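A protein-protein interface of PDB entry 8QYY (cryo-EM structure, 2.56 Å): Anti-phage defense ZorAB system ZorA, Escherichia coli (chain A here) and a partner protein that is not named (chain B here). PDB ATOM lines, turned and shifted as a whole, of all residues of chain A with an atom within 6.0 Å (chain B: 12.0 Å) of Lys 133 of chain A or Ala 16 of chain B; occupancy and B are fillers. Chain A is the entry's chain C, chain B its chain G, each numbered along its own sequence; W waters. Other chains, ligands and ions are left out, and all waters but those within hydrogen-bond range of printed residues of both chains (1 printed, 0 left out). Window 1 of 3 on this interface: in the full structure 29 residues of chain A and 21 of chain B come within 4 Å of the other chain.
Water W1 lies within hydrogen-bond range of the backbone carbonyl oxygen (O) of Lys 133 of chain A (3.2 Å), the backbone carbonyl oxygen (O) of Glu 17 of chain B (3.4 Å) and the backbone NH (N) of Gly 137 of chain A (3.5 Å).
Among the printed residues, pairs that only touch across the chains: Glu 130 of chain A with Arg 11 of chain B (3.8 Å), Glu 130 of chain A with Ser 13 of chain B (3.9 Å), Lys 133 of chain A with Ser 13 of chain B (3.9999 Å), Lys 133 of chain A with Ala 16 of chain B (3.2 Å), His 134 of chain A with Ala 16 of chain B (3.4 Å) and Gly 137 of chain A with Ile 22 of chain B (3.4 Å).
Of chain B, only Arg 11 (3.8 Å) and Ser 13 (3.9 Å) come within 4 Å of Glu 130 of chain A. No residue of chain B comes within 4 Å of Phe 131 of chain A. Of the printed residues of chain B, Lys 133 of chain A touches Ser 13 (3.9999 Å) and Ala 16 (3.2 Å). No residue of chain B comes within 4 Å of Pro 136 of chain A. Of the printed residues of chain B, Gly 137 of chain A touches Ile 22. Lys 199 of chain A touches none of the printed residues of chain B. Printed residues of chain A within 4 Å of Arg 11 of chain B: Glu 130. Printed residues of chain A within 4 Å of Ser 13 of chain B: Glu 130 and Lys 133. Glu 15 of chain B touches none of the printed residues of chain A. Ala 16 of chain B touches just these residues of chain A: Lys 133 and His 134. The nearest printed residue of chain B that does not touch Lys 133 of chain A is Asp 14 of chain B (4.1 Å). The nearest printed residue of chain A that does not touch Ala 16 of chain B is Leu 135 of chain A (6.2 Å).
The side-chain carboxylate of Glu 130 of chain A is in salt-bridge range of the side-chain amino group of Lys 133 of chain A, 3.5 Å away. O of Glu 130 of chain A lies within hydrogen-bond range of ND1 of His 134 of chain A (3.2 Å). The backbone NH of Lys 133 of chain A lies within hydrogen-bond range of the side-chain carboxylate of Glu 198 of chain A (3.1 Å).
Hydrophobic or aromatic side chains of chain B that line the printed part of chain A: Ala 16 and Ile 22.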
ATOM      1  N   ASN A 128     -42.206  -9.753 -14.240  1.00  0.00           N
ATOM      2  CA  ASN A 128     -41.506  -8.478 -14.382  1.00  0.00           C
ATOM      3  C   ASN A 128     -39.993  -8.673 -14.379  1.00  0.00           C
ATOM      4  O   ASN A 128     -39.254  -7.942 -13.721  1.00  0.00           O
ATOM      5  CB  ASN A 128     -41.921  -7.485 -13.296  1.00  0.00           C
ATOM      6  CG  ASN A 128     -43.372  -7.081 -13.397  1.00  0.00           C
ATOM      7  OD1 ASN A 128     -43.740  -6.255 -14.227  1.00  0.00           O
ATOM      8  ND2 ASN A 128     -44.204  -7.652 -12.540  1.00  0.00           N
ATOM      9  N   THR A 129     -39.529  -9.676 -15.129  1.00  0.00           N
ATOM     10  CA  THR A 129     -38.100  -9.953 -15.192  1.00  0.00           C
ATOM     11  C   THR A 129     -37.312  -8.800 -15.793  1.00  0.00           C
ATOM     12  O   THR A 129     -36.111  -8.687 -15.534  1.00  0.00           O
ATOM     13  CB  THR A 129     -37.837 -11.224 -15.998  1.00  0.00           C
ATOM     14  OG1 THR A 129     -38.118 -10.983 -17.381  1.00  0.00           O
ATOM     15  CG2 THR A 129     -38.706 -12.362 -15.502  1.00  0.00           C
ATOM     16  N   GLU A 130     -37.954  -7.936 -16.583  1.00  0.00           N
ATOM     17  CA  GLU A 130     -37.257  -6.787 -17.147  1.00  0.00           C
ATOM     18  C   GLU A 130     -36.810  -5.803 -16.077  1.00  0.00           C
ATOM     19  O   GLU A 130     -35.936  -4.974 -16.343  1.00  0.00           O
ATOM     20  CB  GLU A 130     -38.140  -6.077 -18.172  1.00  0.00           C
ATOM     21  CG  GLU A 130     -38.284  -6.822 -19.488  1.00  0.00           C
ATOM     22  CD  GLU A 130     -36.969  -6.948 -20.239  1.00  0.00           C
ATOM     23  OE1 GLU A 130     -36.292  -7.986 -20.090  1.00  0.00           O
ATOM     24  OE2 GLU A 130     -36.615  -6.010 -20.982  1.00  0.00           O
ATOM     25  N   PHE A 131     -37.393  -5.868 -14.882  1.00  0.00           N
ATOM     26  CA  PHE A 131     -36.947  -5.076 -13.745  1.00  0.00           C
ATOM     27  C   PHE A 131     -36.123  -5.886 -12.755  1.00  0.00           C
ATOM     28  O   PHE A 131     -35.102  -5.406 -12.259  1.00  0.00           O
ATOM     29  CB  PHE A 131     -38.143  -4.457 -13.015  1.00  0.00           C
ATOM     30  CG  PHE A 131     -37.809  -3.953 -11.639  1.00  0.00           C
ATOM     31  CD1 PHE A 131     -37.115  -2.769 -11.473  1.00  0.00           C
ATOM     32  CD2 PHE A 131     -38.167  -4.676 -10.516  1.00  0.00           C
ATOM     33  CE1 PHE A 131     -36.795  -2.310 -10.214  1.00  0.00           C
ATOM     34  CE2 PHE A 131     -37.846  -4.221  -9.256  1.00  0.00           C
ATOM     35  CZ  PHE A 131     -37.162  -3.037  -9.106  1.00  0.00           C
ATOM     36  N   PHE A 132     -36.552  -7.111 -12.456  1.00  0.00           N
ATOM     37  CA  PHE A 132     -35.978  -7.854 -11.343  1.00  0.00           C
ATOM     38  C   PHE A 132     -34.603  -8.426 -11.650  1.00  0.00           C
ATOM     39  O   PHE A 132     -33.875  -8.768 -10.716  1.00  0.00           O
ATOM     40  CB  PHE A 132     -36.930  -8.969 -10.919  1.00  0.00           C
ATOM     41  CG  PHE A 132     -37.989  -8.519  -9.958  1.00  0.00           C
ATOM     42  CD1 PHE A 132     -37.668  -8.232  -8.644  1.00  0.00           C
ATOM     43  CD2 PHE A 132     -39.301  -8.372 -10.367  1.00  0.00           C
ATOM     44  CE1 PHE A 132     -38.635  -7.810  -7.757  1.00  0.00           C
ATOM     45  CE2 PHE A 132     -40.272  -7.955  -9.482  1.00  0.00           C
ATOM     46  CZ  PHE A 132     -39.937  -7.677  -8.174  1.00  0.00           C
ATOM     47  N   LYS A 133     -34.224  -8.544 -12.923  1.00  0.00           N
ATOM     48  CA  LYS A 133     -32.866  -8.984 -13.214  1.00  0.00           C
ATOM     49  C   LYS A 133     -31.827  -7.920 -12.891  1.00  0.00           C
ATOM     50  O   LYS A 133     -30.639  -8.247 -12.802  1.00  0.00           O
ATOM     51  CB  LYS A 133     -32.730  -9.409 -14.676  1.00  0.00           C
ATOM     52  CG  LYS A 133     -32.919  -8.299 -15.682  1.00  0.00           C
ATOM     53  CD  LYS A 133     -32.718  -8.817 -17.096  1.00  0.00           C
ATOM     54  CE  LYS A 133     -33.879  -9.685 -17.540  1.00  0.00           C
ATOM     55  NZ  LYS A 133     -33.763 -10.095 -18.965  1.00  0.00           N
ATOM     56  N   HIS A 134     -32.239  -6.668 -12.714  1.00  0.00           N
ATOM     57  CA  HIS A 134     -31.347  -5.580 -12.341  1.00  0.00           C
ATOM     58  C   HIS A 134     -31.389  -5.254 -10.855  1.00  0.00           C
ATOM     59  O   HIS A 134     -30.692  -4.334 -10.421  1.00  0.00           O
ATOM     60  CB  HIS A 134     -31.681  -4.328 -13.157  1.00  0.00           C
ATOM     61  CG  HIS A 134     -31.704  -4.562 -14.634  1.00  0.00           C
ATOM     62  ND1 HIS A 134     -32.858  -4.842 -15.329  1.00  0.00           N
ATOM     63  CD2 HIS A 134     -30.707  -4.549 -15.551  1.00  0.00           C
ATOM     64  CE1 HIS A 134     -32.572  -5.000 -16.609  1.00  0.00           C
ATOM     65  NE2 HIS A 134     -31.275  -4.824 -16.770  1.00  0.00           N
ATOM     66  N   LEU A 135     -32.191  -5.975 -10.074  1.00  0.00           N
ATOM     67  CA  LEU A 135     -32.266  -5.716  -8.639  1.00  0.00           C
ATOM     68  C   LEU A 135     -30.959  -5.967  -7.889  1.00  0.00           C
ATOM     69  O   LEU A 135     -30.615  -5.141  -7.027  1.00  0.00           O
ATOM     70  CB  LEU A 135     -33.409  -6.539  -8.030  1.00  0.00           C
ATOM     71  CG  LEU A 135     -33.741  -6.242  -6.569  1.00  0.00           C
ATOM     72  CD1 LEU A 135     -34.250  -4.823  -6.429  1.00  0.00           C
ATOM     73  CD2 LEU A 135     -34.765  -7.229  -6.049  1.00  0.00           C
ATOM     74  N   PRO A 136     -30.219  -7.064  -8.116  1.00  0.00           N
ATOM     75  CA  PRO A 136     -28.974  -7.261  -7.350  1.00  0.00           C
ATOM     76  C   PRO A 136     -27.964  -6.139  -7.516  1.00  0.00           C
ATOM     77  O   PRO A 136     -27.264  -5.784  -6.556  1.00  0.00           O
ATOM     78  CB  PRO A 136     -28.440  -8.590  -7.902  1.00  0.00           C
ATOM     79  CG  PRO A 136     -29.637  -9.287  -8.404  1.00  0.00           C
ATOM     80  CD  PRO A 136     -30.520  -8.234  -8.962  1.00  0.00           C
ATOM     81  N   GLY A 137     -27.863  -5.571  -8.717  1.00  0.00           N
ATOM     82  CA  GLY A 137     -27.007  -4.414  -8.903  1.00  0.00           C
ATOM     83  C   GLY A 137     -27.469  -3.226  -8.084  1.00  0.00           C
ATOM     84  O   GLY A 137     -26.654  -2.485  -7.537  1.00  0.00           O
ATOM     85  N   GLU A 198     -33.623 -15.939  -8.045  1.00  0.00           N
ATOM     86  CA  GLU A 198     -34.207 -15.492  -9.302  1.00  0.00           C
ATOM     87  C   GLU A 198     -33.826 -16.403 -10.456  1.00  0.00           C
ATOM     88  O   GLU A 198     -34.684 -16.806 -11.248  1.00  0.00           O
ATOM     89  CB  GLU A 198     -33.750 -14.070  -9.601  1.00  0.00           C
ATOM     90  CG  GLU A 198     -34.363 -13.508 -10.846  1.00  0.00           C
ATOM     91  CD  GLU A 198     -33.942 -12.092 -11.107  1.00  0.00           C
ATOM     92  OE1 GLU A 198     -33.144 -11.551 -10.314  1.00  0.00           O
ATOM     93  OE2 GLU A 198     -34.399 -11.528 -12.119  1.00  0.00           O
ATOM     94  N   LYS A 199     -32.538 -16.715 -10.589  1.00  0.00           N
ATOM     95  CA  LYS A 199     -32.101 -17.521 -11.717  1.00  0.00           C
ATOM     96  C   LYS A 199     -32.606 -18.952 -11.598  1.00  0.00           C
ATOM     97  O   LYS A 199     -33.000 -19.562 -12.599  1.00  0.00           O
ATOM     98  CB  LYS A 199     -30.581 -17.472 -11.827  1.00  0.00           C
ATOM     99  CG  LYS A 199     -30.072 -16.093 -12.193  1.00  0.00           C
ATOM    100  CD  LYS A 199     -30.766 -15.581 -13.437  1.00  0.00           C
ATOM    101  CE  LYS A 199     -31.087 -14.101 -13.334  1.00  0.00           C
ATOM    102  NZ  LYS A 199     -29.893 -13.276 -13.032  1.00  0.00           N
ATOM    103  N   LYS B  10     -38.259 -13.702 -28.993  1.00  0.00           N
ATOM    104  CA  LYS B  10     -37.996 -12.989 -27.753  1.00  0.00           C
ATOM    105  C   LYS B  10     -37.474 -11.586 -28.050  1.00  0.00           C
ATOM    106  O   LYS B  10     -36.814 -11.347 -29.064  1.00  0.00           O
ATOM    107  CB  LYS B  10     -36.982 -13.756 -26.905  1.00  0.00           C
ATOM    108  CG  LYS B  10     -37.441 -15.144 -26.486  1.00  0.00           C
ATOM    109  CD  LYS B  10     -38.687 -15.088 -25.622  1.00  0.00           C
ATOM    110  CE  LYS B  10     -38.400 -14.441 -24.279  1.00  0.00           C
ATOM    111  NZ  LYS B  10     -37.452 -15.249 -23.463  1.00  0.00           N
ATOM    112  N   ARG B  11     -37.779 -10.650 -27.153  1.00  0.00           N
ATOM    113  CA  ARG B  11     -37.379  -9.272 -27.391  1.00  0.00           C
ATOM    114  C   ARG B  11     -35.865  -9.119 -27.252  1.00  0.00           C
ATOM    115  O   ARG B  11     -35.139 -10.057 -26.910  1.00  0.00           O
ATOM    116  CB  ARG B  11     -38.054  -8.306 -26.415  1.00  0.00           C
ATOM    117  CG  ARG B  11     -37.639  -8.493 -24.963  1.00  0.00           C
ATOM    118  CD  ARG B  11     -38.309  -7.472 -24.050  1.00  0.00           C
ATOM    119  NE  ARG B  11     -39.760  -7.577 -23.970  1.00  0.00           N
ATOM    120  CZ  ARG B  11     -40.406  -8.350 -23.108  1.00  0.00           C
ATOM    121  NH1 ARG B  11     -39.757  -9.116 -22.246  1.00  0.00           N
ATOM    122  NH2 ARG B  11     -41.734  -8.339 -23.097  1.00  0.00           N
ATOM    123  N   ARG B  12     -35.397  -7.903 -27.520  1.00  0.00           N
ATOM    124  CA  ARG B  12     -34.013  -7.534 -27.255  1.00  0.00           C
ATOM    125  C   ARG B  12     -33.836  -7.305 -25.760  1.00  0.00           C
ATOM    126  O   ARG B  12     -33.943  -6.171 -25.280  1.00  0.00           O
ATOM    127  CB  ARG B  12     -33.633  -6.284 -28.054  1.00  0.00           C
ATOM    128  CG  ARG B  12     -32.213  -5.790 -27.835  1.00  0.00           C
ATOM    129  CD  ARG B  12     -31.199  -6.789 -28.349  1.00  0.00           C
ATOM    130  NE  ARG B  12     -31.275  -6.944 -29.795  1.00  0.00           N
ATOM    131  CZ  ARG B  12     -30.674  -7.910 -30.474  1.00  0.00           C
ATOM    132  NH1 ARG B  12     -29.931  -8.820 -29.867  1.00  0.00           N
ATOM    133  NH2 ARG B  12     -30.819  -7.964 -31.795  1.00  0.00           N
ATOM    134  N   SER B  13     -33.584  -8.376 -25.013  1.00  0.00           N
ATOM    135  CA  SER B  13     -33.481  -8.314 -23.556  1.00  0.00           C
ATOM    136  C   SER B  13     -32.013  -8.149 -23.184  1.00  0.00           C
ATOM    137  O   SER B  13     -31.274  -9.130 -23.077  1.00  0.00           O
ATOM    138  CB  SER B  13     -34.083  -9.560 -22.916  1.00  0.00           C
ATOM    139  OG  SER B  13     -33.439 -10.733 -23.379  1.00  0.00           O
ATOM    140  N   ASP B  14     -31.592  -6.902 -22.989  1.00  0.00           N
ATOM    141  CA  ASP B  14     -30.223  -6.641 -22.567  1.00  0.00           C
ATOM    142  C   ASP B  14     -30.001  -7.167 -21.155  1.00  0.00           C
ATOM    143  O   ASP B  14     -30.851  -7.010 -20.273  1.00  0.00           O
ATOM    144  CB  ASP B  14     -29.919  -5.143 -22.630  1.00  0.00           C
ATOM    145  CG  ASP B  14     -30.668  -4.348 -21.580  1.00  0.00           C
ATOM    146  OD1 ASP B  14     -31.881  -4.584 -21.410  1.00  0.00           O
ATOM    147  OD2 ASP B  14     -30.042  -3.493 -20.920  1.00  0.00           O
ATOM    148  N   GLU B  15     -28.859  -7.806 -20.947  1.00  0.00           N
ATOM    149  CA  GLU B  15     -28.576  -8.381 -19.646  1.00  0.00           C
ATOM    150  C   GLU B  15     -28.205  -7.289 -18.650  1.00  0.00           C
ATOM    151  O   GLU B  15     -27.855  -6.164 -19.016  1.00  0.00           O
ATOM    152  CB  GLU B  15     -27.459  -9.420 -19.744  1.00  0.00           C
ATOM    153  CG  GLU B  15     -27.954 -10.827 -20.048  1.00  0.00           C
ATOM    154  CD  GLU B  15     -28.475 -11.553 -18.819  1.00  0.00           C
ATOM    155  OE1 GLU B  15     -28.590 -10.919 -17.750  1.00  0.00           O
ATOM    156  OE2 GLU B  15     -28.775 -12.761 -18.927  1.00  0.00           O
ATOM    157  N   ALA B  16     -28.299  -7.635 -17.372  1.00  0.00           N
ATOM    158  CA  ALA B  16     -27.986  -6.687 -16.318  1.00  0.00           C
ATOM    159  C   ALA B  16     -26.478  -6.508 -16.184  1.00  0.00           C
ATOM    160  O   ALA B  16     -25.681  -7.247 -16.767  1.00  0.00           O
ATOM    161  CB  ALA B  16     -28.577  -7.153 -14.990  1.00  0.00           C
ATOM    162  N   GLU B  17     -26.095  -5.499 -15.408  1.00  0.00           N
ATOM    163  CA  GLU B  17     -24.699  -5.330 -15.035  1.00  0.00           C
ATOM    164  C   GLU B  17     -24.187  -6.593 -14.353  1.00  0.00           C
ATOM    165  O   GLU B  17     -24.876  -7.189 -13.521  1.00  0.00           O
ATOM    166  CB  GLU B  17     -24.540  -4.134 -14.096  1.00  0.00           C
ATOM    167  CG  GLU B  17     -24.447  -2.784 -14.777  1.00  0.00           C
ATOM    168  CD  GLU B  17     -23.032  -2.440 -15.195  1.00  0.00           C
ATOM    169  OE1 GLU B  17     -22.815  -1.312 -15.686  1.00  0.00           O
ATOM    170  OE2 GLU B  17     -22.136  -3.292 -15.028  1.00  0.00           O
ATOM    171  N   LYS B  18     -22.980  -7.004 -14.718  1.00  0.00           N
ATOM    172  CA  LYS B  18     -22.381  -8.159 -14.070  1.00  0.00           C
ATOM    173  C   LYS B  18     -22.125  -7.831 -12.603  1.00  0.00           C
ATOM    174  O   LYS B  18     -21.429  -6.851 -12.305  1.00  0.00           O
ATOM    175  CB  LYS B  18     -21.082  -8.556 -14.765  1.00  0.00           C
ATOM    176  CG  LYS B  18     -21.198  -8.631 -16.271  1.00  0.00           C
ATOM    177  CD  LYS B  18     -19.907  -9.115 -16.900  1.00  0.00           C
ATOM    178  CE  LYS B  18     -19.600 -10.547 -16.502  1.00  0.00           C
ATOM    179  NZ  LYS B  18     -18.367 -11.047 -17.167  1.00  0.00           N
ATOM    180  N   PRO B  19     -22.672  -8.608 -11.667  1.00  0.00           N
ATOM    181  CA  PRO B  19     -22.568  -8.226 -10.252  1.00  0.00           C
ATOM    182  C   PRO B  19     -21.146  -8.191  -9.734  1.00  0.00           C
ATOM    183  O   PRO B  19     -20.867  -7.485  -8.754  1.00  0.00           O
ATOM    184  CB  PRO B  19     -23.399  -9.303  -9.543  1.00  0.00           C
ATOM    185  CG  PRO B  19     -23.341 -10.478 -10.456  1.00  0.00           C
ATOM    186  CD  PRO B  19     -23.324  -9.915 -11.845  1.00  0.00           C
ATOM    187  N   PHE B  20     -20.232  -8.930 -10.365  1.00  0.00           N
ATOM    188  CA  PHE B  20     -18.871  -8.989  -9.852  1.00  0.00           C
ATOM    189  C   PHE B  20     -18.208  -7.624  -9.896  1.00  0.00           C
ATOM    190  O   PHE B  20     -17.466  -7.264  -8.982  1.00  0.00           O
ATOM    191  CB  PHE B  20     -18.031  -9.995 -10.632  1.00  0.00           C
ATOM    192  CG  PHE B  20     -16.555  -9.813 -10.430  1.00  0.00           C
ATOM    193  CD1 PHE B  20     -15.984 -10.027  -9.188  1.00  0.00           C
ATOM    194  CD2 PHE B  20     -15.744  -9.404 -11.469  1.00  0.00           C
ATOM    195  CE1 PHE B  20     -14.634  -9.849  -8.991  1.00  0.00           C
ATOM    196  CE2 PHE B  20     -14.389  -9.228 -11.275  1.00  0.00           C
ATOM    197  CZ  PHE B  20     -13.835  -9.449 -10.035  1.00  0.00           C
ATOM    198  N   TRP B  21     -18.455  -6.850 -10.950  1.00  0.00           N
ATOM    199  CA  TRP B  21     -17.755  -5.579 -11.094  1.00  0.00           C
ATOM    200  C   TRP B  21     -18.225  -4.558 -10.066  1.00  0.00           C
ATOM    201  O   TRP B  21     -17.406  -3.844  -9.478  1.00  0.00           O
ATOM    202  CB  TRP B  21     -17.927  -5.053 -12.512  1.00  0.00           C
ATOM    203  CG  TRP B  21     -17.122  -5.831 -13.482  1.00  0.00           C
ATOM    204  CD1 TRP B  21     -17.589  -6.615 -14.491  1.00  0.00           C
ATOM    205  CD2 TRP B  21     -15.698  -5.932 -13.517  1.00  0.00           C
ATOM    206  NE1 TRP B  21     -16.541  -7.187 -15.165  1.00  0.00           N
ATOM    207  CE2 TRP B  21     -15.368  -6.784 -14.585  1.00  0.00           C
ATOM    208  CE3 TRP B  21     -14.667  -5.376 -12.754  1.00  0.00           C
ATOM    209  CZ2 TRP B  21     -14.054  -7.093 -14.909  1.00  0.00           C
ATOM    210  CZ3 TRP B  21     -13.368  -5.686 -13.077  1.00  0.00           C
ATOM    211  CH2 TRP B  21     -13.072  -6.532 -14.146  1.00  0.00           C
ATOM    212  N   ILE B  22     -19.533  -4.479  -9.825  1.00  0.00           N
ATOM    213  CA  ILE B  22     -20.028  -3.550  -8.817  1.00  0.00           C
ATOM    214  C   ILE B  22     -19.625  -4.011  -7.418  1.00  0.00           C
ATOM    215  O   ILE B  22     -19.279  -3.191  -6.557  1.00  0.00           O
ATOM    216  CB  ILE B  22     -21.550  -3.362  -8.963  1.00  0.00           C
ATOM    217  CG1 ILE B  22     -22.063  -2.318  -7.974  1.00  0.00           C
ATOM    218  CG2 ILE B  22     -22.291  -4.674  -8.797  1.00  0.00           C
ATOM    219  CD1 ILE B  22     -23.431  -1.794  -8.317  1.00  0.00           C
ATOM    220  N   SER B  23     -19.635  -5.325  -7.171  1.00  0.00           N
ATOM    221  CA  SER B  23     -19.179  -5.832  -5.879  1.00  0.00           C
ATOM    222  C   SER B  23     -17.693  -5.567  -5.670  1.00  0.00           C
ATOM    223  O   SER B  23     -17.260  -5.252  -4.556  1.00  0.00           O
ATOM    224  CB  SER B  23     -19.477  -7.325  -5.766  1.00  0.00           C
ATOM    225  OG  SER B  23     -20.865  -7.578  -5.858  1.00  0.00           O
HETATM  226  O   HOH W   1     -27.806  -7.309 -11.744  1.00  0.00           O
